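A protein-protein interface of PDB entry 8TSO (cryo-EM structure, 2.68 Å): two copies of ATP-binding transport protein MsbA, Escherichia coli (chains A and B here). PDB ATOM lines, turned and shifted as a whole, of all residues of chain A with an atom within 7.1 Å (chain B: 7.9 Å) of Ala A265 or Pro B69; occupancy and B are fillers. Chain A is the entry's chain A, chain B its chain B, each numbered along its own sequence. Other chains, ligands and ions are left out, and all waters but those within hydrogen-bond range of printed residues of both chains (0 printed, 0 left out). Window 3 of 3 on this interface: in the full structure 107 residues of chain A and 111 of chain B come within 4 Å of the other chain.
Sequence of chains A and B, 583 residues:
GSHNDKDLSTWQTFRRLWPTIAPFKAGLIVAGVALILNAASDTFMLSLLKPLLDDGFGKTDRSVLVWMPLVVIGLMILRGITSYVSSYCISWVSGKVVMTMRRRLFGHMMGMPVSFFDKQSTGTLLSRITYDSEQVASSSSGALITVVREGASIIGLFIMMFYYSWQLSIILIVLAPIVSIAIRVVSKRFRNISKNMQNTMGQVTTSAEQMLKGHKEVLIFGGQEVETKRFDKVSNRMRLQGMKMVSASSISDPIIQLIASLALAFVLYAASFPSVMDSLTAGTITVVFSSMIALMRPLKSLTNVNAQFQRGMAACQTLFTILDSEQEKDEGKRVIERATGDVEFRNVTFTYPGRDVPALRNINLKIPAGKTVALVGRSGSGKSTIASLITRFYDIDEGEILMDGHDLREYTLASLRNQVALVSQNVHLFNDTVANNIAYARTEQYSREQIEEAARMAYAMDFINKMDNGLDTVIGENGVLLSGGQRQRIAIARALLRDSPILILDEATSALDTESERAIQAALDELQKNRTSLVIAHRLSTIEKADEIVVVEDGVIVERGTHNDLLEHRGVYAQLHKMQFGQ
The side-chain hydroxyl (OG) of Ser A272 lies within hydrogen-bond range of the backbone carbonyl oxygen (O) of Tyr A269, at 2.7 Å.
No position is printed for both chains.
Ala A265 touches just one residue of chain B: Pro B69. Printed residues of chain A within 4 Å of Pro B69: Ala A265, Leu A268 and Tyr A269. Printed residues of chain A within 4 Å of Val B72: Leu A268. Of the printed residues of chain B, Ala A271 touches Leu B65 (3.999 Å). Met A292 touches none of the printed residues of chain B. Gly B74 touches none of the printed residues of chain A.
Hydrophobic or aromatic side chains of chain A that line the printed part of chain B: Leu A262, Ala A265 and Leu A268. Of the 14 printed residues of chain B, 5 touch a printed residue of chain A. Hydrophobic or aromatic side chains of chain B that line the printed part of chain A: Leu B65, Pro B69, Val B72, Ile B73 and Met B76. Along chain B the printed residues that touch a printed residue of chain A span positions 65 to 76. Among the printed residues, no Asp or Glu carboxylate lies within 4 Å of a Lys or Arg side-chain nitrogen of the other chain.
Among the printed residues, merely in contact across the chains: Ser A261 with Met B76 (3.3 Å), Ala A265 with Pro B69 (3.5 Å), Leu A268 with Leu B65 (3.6 Å), Leu A262 with Ile B73 (3.6 Å), Leu A268 with Val B72 (3.7 Å), Tyr A269 with Pro B69 (3.7 Å), Leu A268 with Pro B69 (3.996 Å) and Ala A271 with Leu B65 (3.999 Å).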
ATOM      1  N   ALA A 260     -25.787   0.292  24.447  1.00  0.00           N
ATOM      2  CA  ALA A 260     -25.687  -0.509  23.231  1.00  0.00           C
ATOM      3  C   ALA A 260     -26.018  -1.973  23.498  1.00  0.00           C
ATOM      4  O   ALA A 260     -26.743  -2.603  22.718  1.00  0.00           O
ATOM      5  CB  ALA A 260     -24.291  -0.377  22.628  1.00  0.00           C
ATOM      6  N   SER A 261     -25.496  -2.532  24.592  1.00  0.00           N
ATOM      7  CA  SER A 261     -25.765  -3.923  24.937  1.00  0.00           C
ATOM      8  C   SER A 261     -27.205  -4.153  25.371  1.00  0.00           C
ATOM      9  O   SER A 261     -27.637  -5.311  25.444  1.00  0.00           O
ATOM     10  CB  SER A 261     -24.821  -4.383  26.044  1.00  0.00           C
ATOM     11  OG  SER A 261     -25.131  -3.743  27.268  1.00  0.00           O
ATOM     12  N   LEU A 262     -27.939  -3.088  25.695  1.00  0.00           N
ATOM     13  CA  LEU A 262     -29.377  -3.230  25.903  1.00  0.00           C
ATOM     14  C   LEU A 262     -30.054  -3.845  24.683  1.00  0.00           C
ATOM     15  O   LEU A 262     -31.017  -4.609  24.825  1.00  0.00           O
ATOM     16  CB  LEU A 262     -29.998  -1.872  26.227  1.00  0.00           C
ATOM     17  CG  LEU A 262     -30.898  -1.767  27.457  1.00  0.00           C
ATOM     18  CD1 LEU A 262     -30.223  -2.372  28.672  1.00  0.00           C
ATOM     19  CD2 LEU A 262     -31.267  -0.318  27.714  1.00  0.00           C
ATOM     20  N   ALA A 263     -29.558  -3.540  23.483  1.00  0.00           N
ATOM     21  CA  ALA A 263     -30.108  -4.137  22.270  1.00  0.00           C
ATOM     22  C   ALA A 263     -29.867  -5.641  22.225  1.00  0.00           C
ATOM     23  O   ALA A 263     -30.764  -6.407  21.854  1.00  0.00           O
ATOM     24  CB  ALA A 263     -29.508  -3.463  21.037  1.00  0.00           C
ATOM     25  N   LEU A 264     -28.660  -6.085  22.583  1.00  0.00           N
ATOM     26  CA  LEU A 264     -28.391  -7.519  22.629  1.00  0.00           C
ATOM     27  C   LEU A 264     -29.242  -8.201  23.687  1.00  0.00           C
ATOM     28  O   LEU A 264     -29.710  -9.328  23.488  1.00  0.00           O
ATOM     29  CB  LEU A 264     -26.907  -7.776  22.890  1.00  0.00           C
ATOM     30  CG  LEU A 264     -25.910  -7.092  21.960  1.00  0.00           C
ATOM     31  CD1 LEU A 264     -24.704  -6.596  22.734  1.00  0.00           C
ATOM     32  CD2 LEU A 264     -25.489  -8.051  20.871  1.00  0.00           C
ATOM     33  N   ALA A 265     -29.442  -7.538  24.827  1.00  0.00           N
ATOM     34  CA  ALA A 265     -30.322  -8.090  25.852  1.00  0.00           C
ATOM     35  C   ALA A 265     -31.742  -8.251  25.324  1.00  0.00           C
ATOM     36  O   ALA A 265     -32.390  -9.276  25.565  1.00  0.00           O
ATOM     37  CB  ALA A 265     -30.306  -7.200  27.093  1.00  0.00           C
ATOM     38  N   PHE A 266     -32.239  -7.249  24.594  1.00  0.00           N
ATOM     39  CA  PHE A 266     -33.572  -7.349  24.008  1.00  0.00           C
ATOM     40  C   PHE A 266     -33.648  -8.480  22.991  1.00  0.00           C
ATOM     41  O   PHE A 266     -34.646  -9.208  22.936  1.00  0.00           O
ATOM     42  CB  PHE A 266     -33.963  -6.028  23.352  1.00  0.00           C
ATOM     43  CG  PHE A 266     -35.122  -6.144  22.404  1.00  0.00           C
ATOM     44  CD1 PHE A 266     -36.405  -6.340  22.880  1.00  0.00           C
ATOM     45  CD2 PHE A 266     -34.925  -6.074  21.036  1.00  0.00           C
ATOM     46  CE1 PHE A 266     -37.472  -6.451  22.010  1.00  0.00           C
ATOM     47  CE2 PHE A 266     -35.986  -6.184  20.161  1.00  0.00           C
ATOM     48  CZ  PHE A 266     -37.261  -6.374  20.648  1.00  0.00           C
ATOM     49  N   VAL A 267     -32.611  -8.632  22.165  1.00  0.00           N
ATOM     50  CA  VAL A 267     -32.610  -9.694  21.162  1.00  0.00           C
ATOM     51  C   VAL A 267     -32.626 -11.061  21.831  1.00  0.00           C
ATOM     52  O   VAL A 267     -33.361 -11.964  21.414  1.00  0.00           O
ATOM     53  CB  VAL A 267     -31.403  -9.536  20.217  1.00  0.00           C
ATOM     54  CG1 VAL A 267     -31.159 -10.819  19.441  1.00  0.00           C
ATOM     55  CG2 VAL A 267     -31.632  -8.377  19.273  1.00  0.00           C
ATOM     56  N   LEU A 268     -31.819 -11.235  22.880  1.00  0.00           N
ATOM     57  CA  LEU A 268     -31.809 -12.502  23.603  1.00  0.00           C
ATOM     58  C   LEU A 268     -33.144 -12.769  24.287  1.00  0.00           C
ATOM     59  O   LEU A 268     -33.601 -13.917  24.322  1.00  0.00           O
ATOM     60  CB  LEU A 268     -30.677 -12.518  24.627  1.00  0.00           C
ATOM     61  CG  LEU A 268     -29.263 -12.681  24.069  1.00  0.00           C
ATOM     62  CD1 LEU A 268     -28.235 -12.216  25.083  1.00  0.00           C
ATOM     63  CD2 LEU A 268     -29.001 -14.116  23.657  1.00  0.00           C
ATOM     64  N   TYR A 269     -33.776 -11.733  24.843  1.00  0.00           N
ATOM     65  CA  TYR A 269     -35.091 -11.910  25.451  1.00  0.00           C
ATOM     66  C   TYR A 269     -36.131 -12.314  24.415  1.00  0.00           C
ATOM     67  O   TYR A 269     -36.984 -13.168  24.682  1.00  0.00           O
ATOM     68  CB  TYR A 269     -35.512 -10.624  26.162  1.00  0.00           C
ATOM     69  CG  TYR A 269     -36.866 -10.706  26.826  1.00  0.00           C
ATOM     70  CD1 TYR A 269     -37.071 -11.525  27.927  1.00  0.00           C
ATOM     71  CD2 TYR A 269     -37.936  -9.959  26.357  1.00  0.00           C
ATOM     72  CE1 TYR A 269     -38.304 -11.602  28.539  1.00  0.00           C
ATOM     73  CE2 TYR A 269     -39.175 -10.029  26.964  1.00  0.00           C
ATOM     74  CZ  TYR A 269     -39.352 -10.853  28.054  1.00  0.00           C
ATOM     75  OH  TYR A 269     -40.583 -10.927  28.663  1.00  0.00           O
ATOM     76  N   ALA A 270     -36.081 -11.706  23.228  1.00  0.00           N
ATOM     77  CA  ALA A 270     -37.026 -12.056  22.173  1.00  0.00           C
ATOM     78  C   ALA A 270     -36.783 -13.468  21.656  1.00  0.00           C
ATOM     79  O   ALA A 270     -37.730 -14.178  21.299  1.00  0.00           O
ATOM     80  CB  ALA A 270     -36.935 -11.044  21.032  1.00  0.00           C
ATOM     81  N   ALA A 271     -35.520 -13.892  21.602  1.00  0.00           N
ATOM     82  CA  ALA A 271     -35.186 -15.225  21.114  1.00  0.00           C
ATOM     83  C   ALA A 271     -35.594 -16.332  22.074  1.00  0.00           C
ATOM     84  O   ALA A 271     -35.528 -17.506  21.693  1.00  0.00           O
ATOM     85  CB  ALA A 271     -33.687 -15.318  20.830  1.00  0.00           C
ATOM     86  N   SER A 272     -36.003 -16.003  23.295  1.00  0.00           N
ATOM     87  CA  SER A 272     -36.438 -16.997  24.265  1.00  0.00           C
ATOM     88  C   SER A 272     -37.901 -17.385  24.095  1.00  0.00           C
ATOM     89  O   SER A 272     -38.374 -18.285  24.796  1.00  0.00           O
ATOM     90  CB  SER A 272     -36.206 -16.484  25.688  1.00  0.00           C
ATOM     91  OG  SER A 272     -37.158 -15.494  26.030  1.00  0.00           O
ATOM     92  N   PHE A 289     -27.690 -10.839  15.967  1.00  0.00           N
ATOM     93  CA  PHE A 289     -26.916 -10.792  17.202  1.00  0.00           C
ATOM     94  C   PHE A 289     -25.441 -10.534  16.915  1.00  0.00           C
ATOM     95  O   PHE A 289     -24.804  -9.690  17.562  1.00  0.00           O
ATOM     96  CB  PHE A 289     -27.105 -12.100  17.973  1.00  0.00           C
ATOM     97  CG  PHE A 289     -26.673 -12.031  19.408  1.00  0.00           C
ATOM     98  CD1 PHE A 289     -27.429 -11.339  20.337  1.00  0.00           C
ATOM     99  CD2 PHE A 289     -25.527 -12.677  19.833  1.00  0.00           C
ATOM    100  CE1 PHE A 289     -27.041 -11.278  21.657  1.00  0.00           C
ATOM    101  CE2 PHE A 289     -25.136 -12.622  21.154  1.00  0.00           C
ATOM    102  CZ  PHE A 289     -25.893 -11.921  22.067  1.00  0.00           C
ATOM    103  N   MET A 292     -24.972  -6.817  15.962  1.00  0.00           N
ATOM    104  CA  MET A 292     -24.855  -5.869  17.074  1.00  0.00           C
ATOM    105  C   MET A 292     -23.558  -6.065  17.856  1.00  0.00           C
ATOM    106  O   MET A 292     -22.974  -5.090  18.357  1.00  0.00           O
ATOM    107  CB  MET A 292     -26.067  -5.939  18.001  1.00  0.00           C
ATOM    108  CG  MET A 292     -27.370  -6.299  17.336  1.00  0.00           C
ATOM    109  SD  MET A 292     -28.725  -5.514  18.225  1.00  0.00           S
ATOM    110  CE  MET A 292     -30.119  -5.897  17.179  1.00  0.00           C
ATOM    111  N   SER B  63     -34.263 -22.192  29.133  1.00  0.00           N
ATOM    112  CA  SER B  63     -34.125 -21.646  30.479  1.00  0.00           C
ATOM    113  C   SER B  63     -32.874 -20.783  30.589  1.00  0.00           C
ATOM    114  O   SER B  63     -32.879 -19.741  31.255  1.00  0.00           O
ATOM    115  CB  SER B  63     -34.096 -22.778  31.505  1.00  0.00           C
ATOM    116  OG  SER B  63     -33.959 -22.270  32.820  1.00  0.00           O
ATOM    117  N   VAL B  64     -31.784 -21.211  29.947  1.00  0.00           N
ATOM    118  CA  VAL B  64     -30.571 -20.399  29.912  1.00  0.00           C
ATOM    119  C   VAL B  64     -30.830 -19.089  29.178  1.00  0.00           C
ATOM    120  O   VAL B  64     -30.408 -18.014  29.624  1.00  0.00           O
ATOM    121  CB  VAL B  64     -29.419 -21.193  29.268  1.00  0.00           C
ATOM    122  CG1 VAL B  64     -28.227 -20.287  29.002  1.00  0.00           C
ATOM    123  CG2 VAL B  64     -29.023 -22.362  30.155  1.00  0.00           C
ATOM    124  N   LEU B  65     -31.535 -19.158  28.046  1.00  0.00           N
ATOM    125  CA  LEU B  65     -31.833 -17.955  27.276  1.00  0.00           C
ATOM    126  C   LEU B  65     -32.698 -16.982  28.065  1.00  0.00           C
ATOM    127  O   LEU B  65     -32.671 -15.774  27.803  1.00  0.00           O
ATOM    128  CB  LEU B  65     -32.521 -18.331  25.965  1.00  0.00           C
ATOM    129  CG  LEU B  65     -31.671 -18.236  24.699  1.00  0.00           C
ATOM    130  CD1 LEU B  65     -32.322 -19.001  23.559  1.00  0.00           C
ATOM    131  CD2 LEU B  65     -31.450 -16.786  24.315  1.00  0.00           C
ATOM    132  N   VAL B  66     -33.475 -17.486  29.024  1.00  0.00           N
ATOM    133  CA  VAL B  66     -34.266 -16.608  29.880  1.00  0.00           C
ATOM    134  C   VAL B  66     -33.355 -15.732  30.732  1.00  0.00           C
ATOM    135  O   VAL B  66     -33.593 -14.529  30.884  1.00  0.00           O
ATOM    136  CB  VAL B  66     -35.231 -17.441  30.743  1.00  0.00           C
ATOM    137  CG1 VAL B  66     -35.779 -16.613  31.895  1.00  0.00           C
ATOM    138  CG2 VAL B  66     -36.364 -17.987  29.890  1.00  0.00           C
ATOM    139  N   TRP B  67     -32.295 -16.316  31.289  1.00  0.00           N
ATOM    140  CA  TRP B  67     -31.375 -15.595  32.157  1.00  0.00           C
ATOM    141  C   TRP B  67     -30.225 -14.935  31.406  1.00  0.00           C
ATOM    142  O   TRP B  67     -29.421 -14.240  32.033  1.00  0.00           O
ATOM    143  CB  TRP B  67     -30.808 -16.540  33.221  1.00  0.00           C
ATOM    144  CG  TRP B  67     -31.825 -16.985  34.226  1.00  0.00           C
ATOM    145  CD1 TRP B  67     -32.643 -18.073  34.135  1.00  0.00           C
ATOM    146  CD2 TRP B  67     -32.135 -16.353  35.474  1.00  0.00           C
ATOM    147  NE1 TRP B  67     -33.443 -18.158  35.249  1.00  0.00           N
ATOM    148  CE2 TRP B  67     -33.151 -17.114  36.086  1.00  0.00           C
ATOM    149  CE3 TRP B  67     -31.652 -15.220  36.134  1.00  0.00           C
ATOM    150  CZ2 TRP B  67     -33.692 -16.778  37.324  1.00  0.00           C
ATOM    151  CZ3 TRP B  67     -32.191 -14.887  37.363  1.00  0.00           C
ATOM    152  CH2 TRP B  67     -33.199 -15.663  37.946  1.00  0.00           C
ATOM    153  N   MET B  68     -30.118 -15.143  30.095  1.00  0.00           N
ATOM    154  CA  MET B  68     -29.044 -14.518  29.326  1.00  0.00           C
ATOM    155  C   MET B  68     -29.043 -12.990  29.361  1.00  0.00           C
ATOM    156  O   MET B  68     -27.957 -12.414  29.540  1.00  0.00           O
ATOM    157  CB  MET B  68     -29.091 -15.007  27.871  1.00  0.00           C
ATOM    158  CG  MET B  68     -28.518 -16.396  27.654  1.00  0.00           C
ATOM    159  SD  MET B  68     -26.721 -16.402  27.537  1.00  0.00           S
ATOM    160  CE  MET B  68     -26.284 -16.993  29.169  1.00  0.00           C
ATOM    161  N   PRO B  69     -30.166 -12.282  29.169  1.00  0.00           N
ATOM    162  CA  PRO B  69     -30.089 -10.807  29.177  1.00  0.00           C
ATOM    163  C   PRO B  69     -29.560 -10.226  30.479  1.00  0.00           C
ATOM    164  O   PRO B  69     -28.790  -9.256  30.458  1.00  0.00           O
ATOM    165  CB  PRO B  69     -31.540 -10.385  28.910  1.00  0.00           C
ATOM    166  CG  PRO B  69     -32.147 -11.537  28.211  1.00  0.00           C
ATOM    167  CD  PRO B  69     -31.520 -12.747  28.817  1.00  0.00           C
ATOM    168  N   LEU B  70     -29.953 -10.797  31.618  1.00  0.00           N
ATOM    169  CA  LEU B  70     -29.458 -10.300  32.897  1.00  0.00           C
ATOM    170  C   LEU B  70     -27.961 -10.535  33.035  1.00  0.00           C
ATOM    171  O   LEU B  70     -27.239  -9.686  33.567  1.00  0.00           O
ATOM    172  CB  LEU B  70     -30.222 -10.957  34.046  1.00  0.00           C
ATOM    173  CG  LEU B  70     -31.733 -11.075  33.841  1.00  0.00           C
ATOM    174  CD1 LEU B  70     -32.343 -12.026  34.853  1.00  0.00           C
ATOM    175  CD2 LEU B  70     -32.392  -9.708  33.920  1.00  0.00           C
ATOM    176  N   VAL B  71     -27.478 -11.682  32.553  1.00  0.00           N
ATOM    177  CA  VAL B  71     -26.044 -11.952  32.571  1.00  0.00           C
ATOM    178  C   VAL B  71     -25.305 -10.951  31.693  1.00  0.00           C
ATOM    179  O   VAL B  71     -24.227 -10.464  32.055  1.00  0.00           O
ATOM    180  CB  VAL B  71     -25.766 -13.402  32.138  1.00  0.00           C
ATOM    181  CG1 VAL B  71     -24.275 -13.637  31.997  1.00  0.00           C
ATOM    182  CG2 VAL B  71     -26.366 -14.374  33.138  1.00  0.00           C
ATOM    183  N   VAL B  72     -25.870 -10.629  30.528  1.00  0.00           N
ATOM    184  CA  VAL B  72     -25.242  -9.652  29.639  1.00  0.00           C
ATOM    185  C   VAL B  72     -25.155  -8.292  30.320  1.00  0.00           C
ATOM    186  O   VAL B  72     -24.113  -7.624  30.288  1.00  0.00           O
ATOM    187  CB  VAL B  72     -26.011  -9.566  28.308  1.00  0.00           C
ATOM    188  CG1 VAL B  72     -25.508  -8.399  27.477  1.00  0.00           C
ATOM    189  CG2 VAL B  72     -25.878 -10.863  27.537  1.00  0.00           C
ATOM    190  N   ILE B  73     -26.249  -7.866  30.955  1.00  0.00           N
ATOM    191  CA  ILE B  73     -26.260  -6.570  31.631  1.00  0.00           C
ATOM    192  C   ILE B  73     -25.245  -6.550  32.768  1.00  0.00           C
ATOM    193  O   ILE B  73     -24.491  -5.582  32.929  1.00  0.00           O
ATOM    194  CB  ILE B  73     -27.677  -6.235  32.132  1.00  0.00           C
ATOM    195  CG1 ILE B  73     -28.646  -6.119  30.956  1.00  0.00           C
ATOM    196  CG2 ILE B  73     -27.670  -4.946  32.930  1.00  0.00           C
ATOM    197  CD1 ILE B  73     -28.198  -5.150  29.894  1.00  0.00           C
ATOM    198  N   GLY B  74     -25.206  -7.615  33.570  1.00  0.00           N
ATOM    199  CA  GLY B  74     -24.260  -7.665  34.671  1.00  0.00           C
ATOM    200  C   GLY B  74     -22.817  -7.658  34.208  1.00  0.00           C
ATOM    201  O   GLY B  74     -21.971  -6.981  34.799  1.00  0.00           O
ATOM    202  N   LEU B  75     -22.513  -8.407  33.146  1.00  0.00           N
ATOM    203  CA  LEU B  75     -21.154  -8.418  32.618  1.00  0.00           C
ATOM    204  C   LEU B  75     -20.764  -7.054  32.068  1.00  0.00           C
ATOM    205  O   LEU B  75     -19.624  -6.611  32.244  1.00  0.00           O
ATOM    206  CB  LEU B  75     -21.016  -9.491  31.539  1.00  0.00           C
ATOM    207  CG  LEU B  75     -20.932 -10.932  32.040  1.00  0.00           C
ATOM    208  CD1 LEU B  75     -20.814 -11.894  30.876  1.00  0.00           C
ATOM    209  CD2 LEU B  75     -19.757 -11.090  32.985  1.00  0.00           C
ATOM    210  N   MET B  76     -21.694  -6.372  31.394  1.00  0.00           N
ATOM    211  CA  MET B  76     -21.395  -5.035  30.896  1.00  0.00           C
ATOM    212  C   MET B  76     -21.149  -4.059  32.041  1.00  0.00           C
ATOM    213  O   MET B  76     -20.246  -3.219  31.966  1.00  0.00           O
ATOM    214  CB  MET B  76     -22.528  -4.547  29.996  1.00  0.00           C
ATOM    215  CG  MET B  76     -22.529  -5.185  28.617  1.00  0.00           C
ATOM    216  SD  MET B  76     -20.887  -5.338  27.889  1.00  0.00           S
ATOM    217  CE  MET B  76     -20.651  -3.687  27.244  1.00  0.00           C
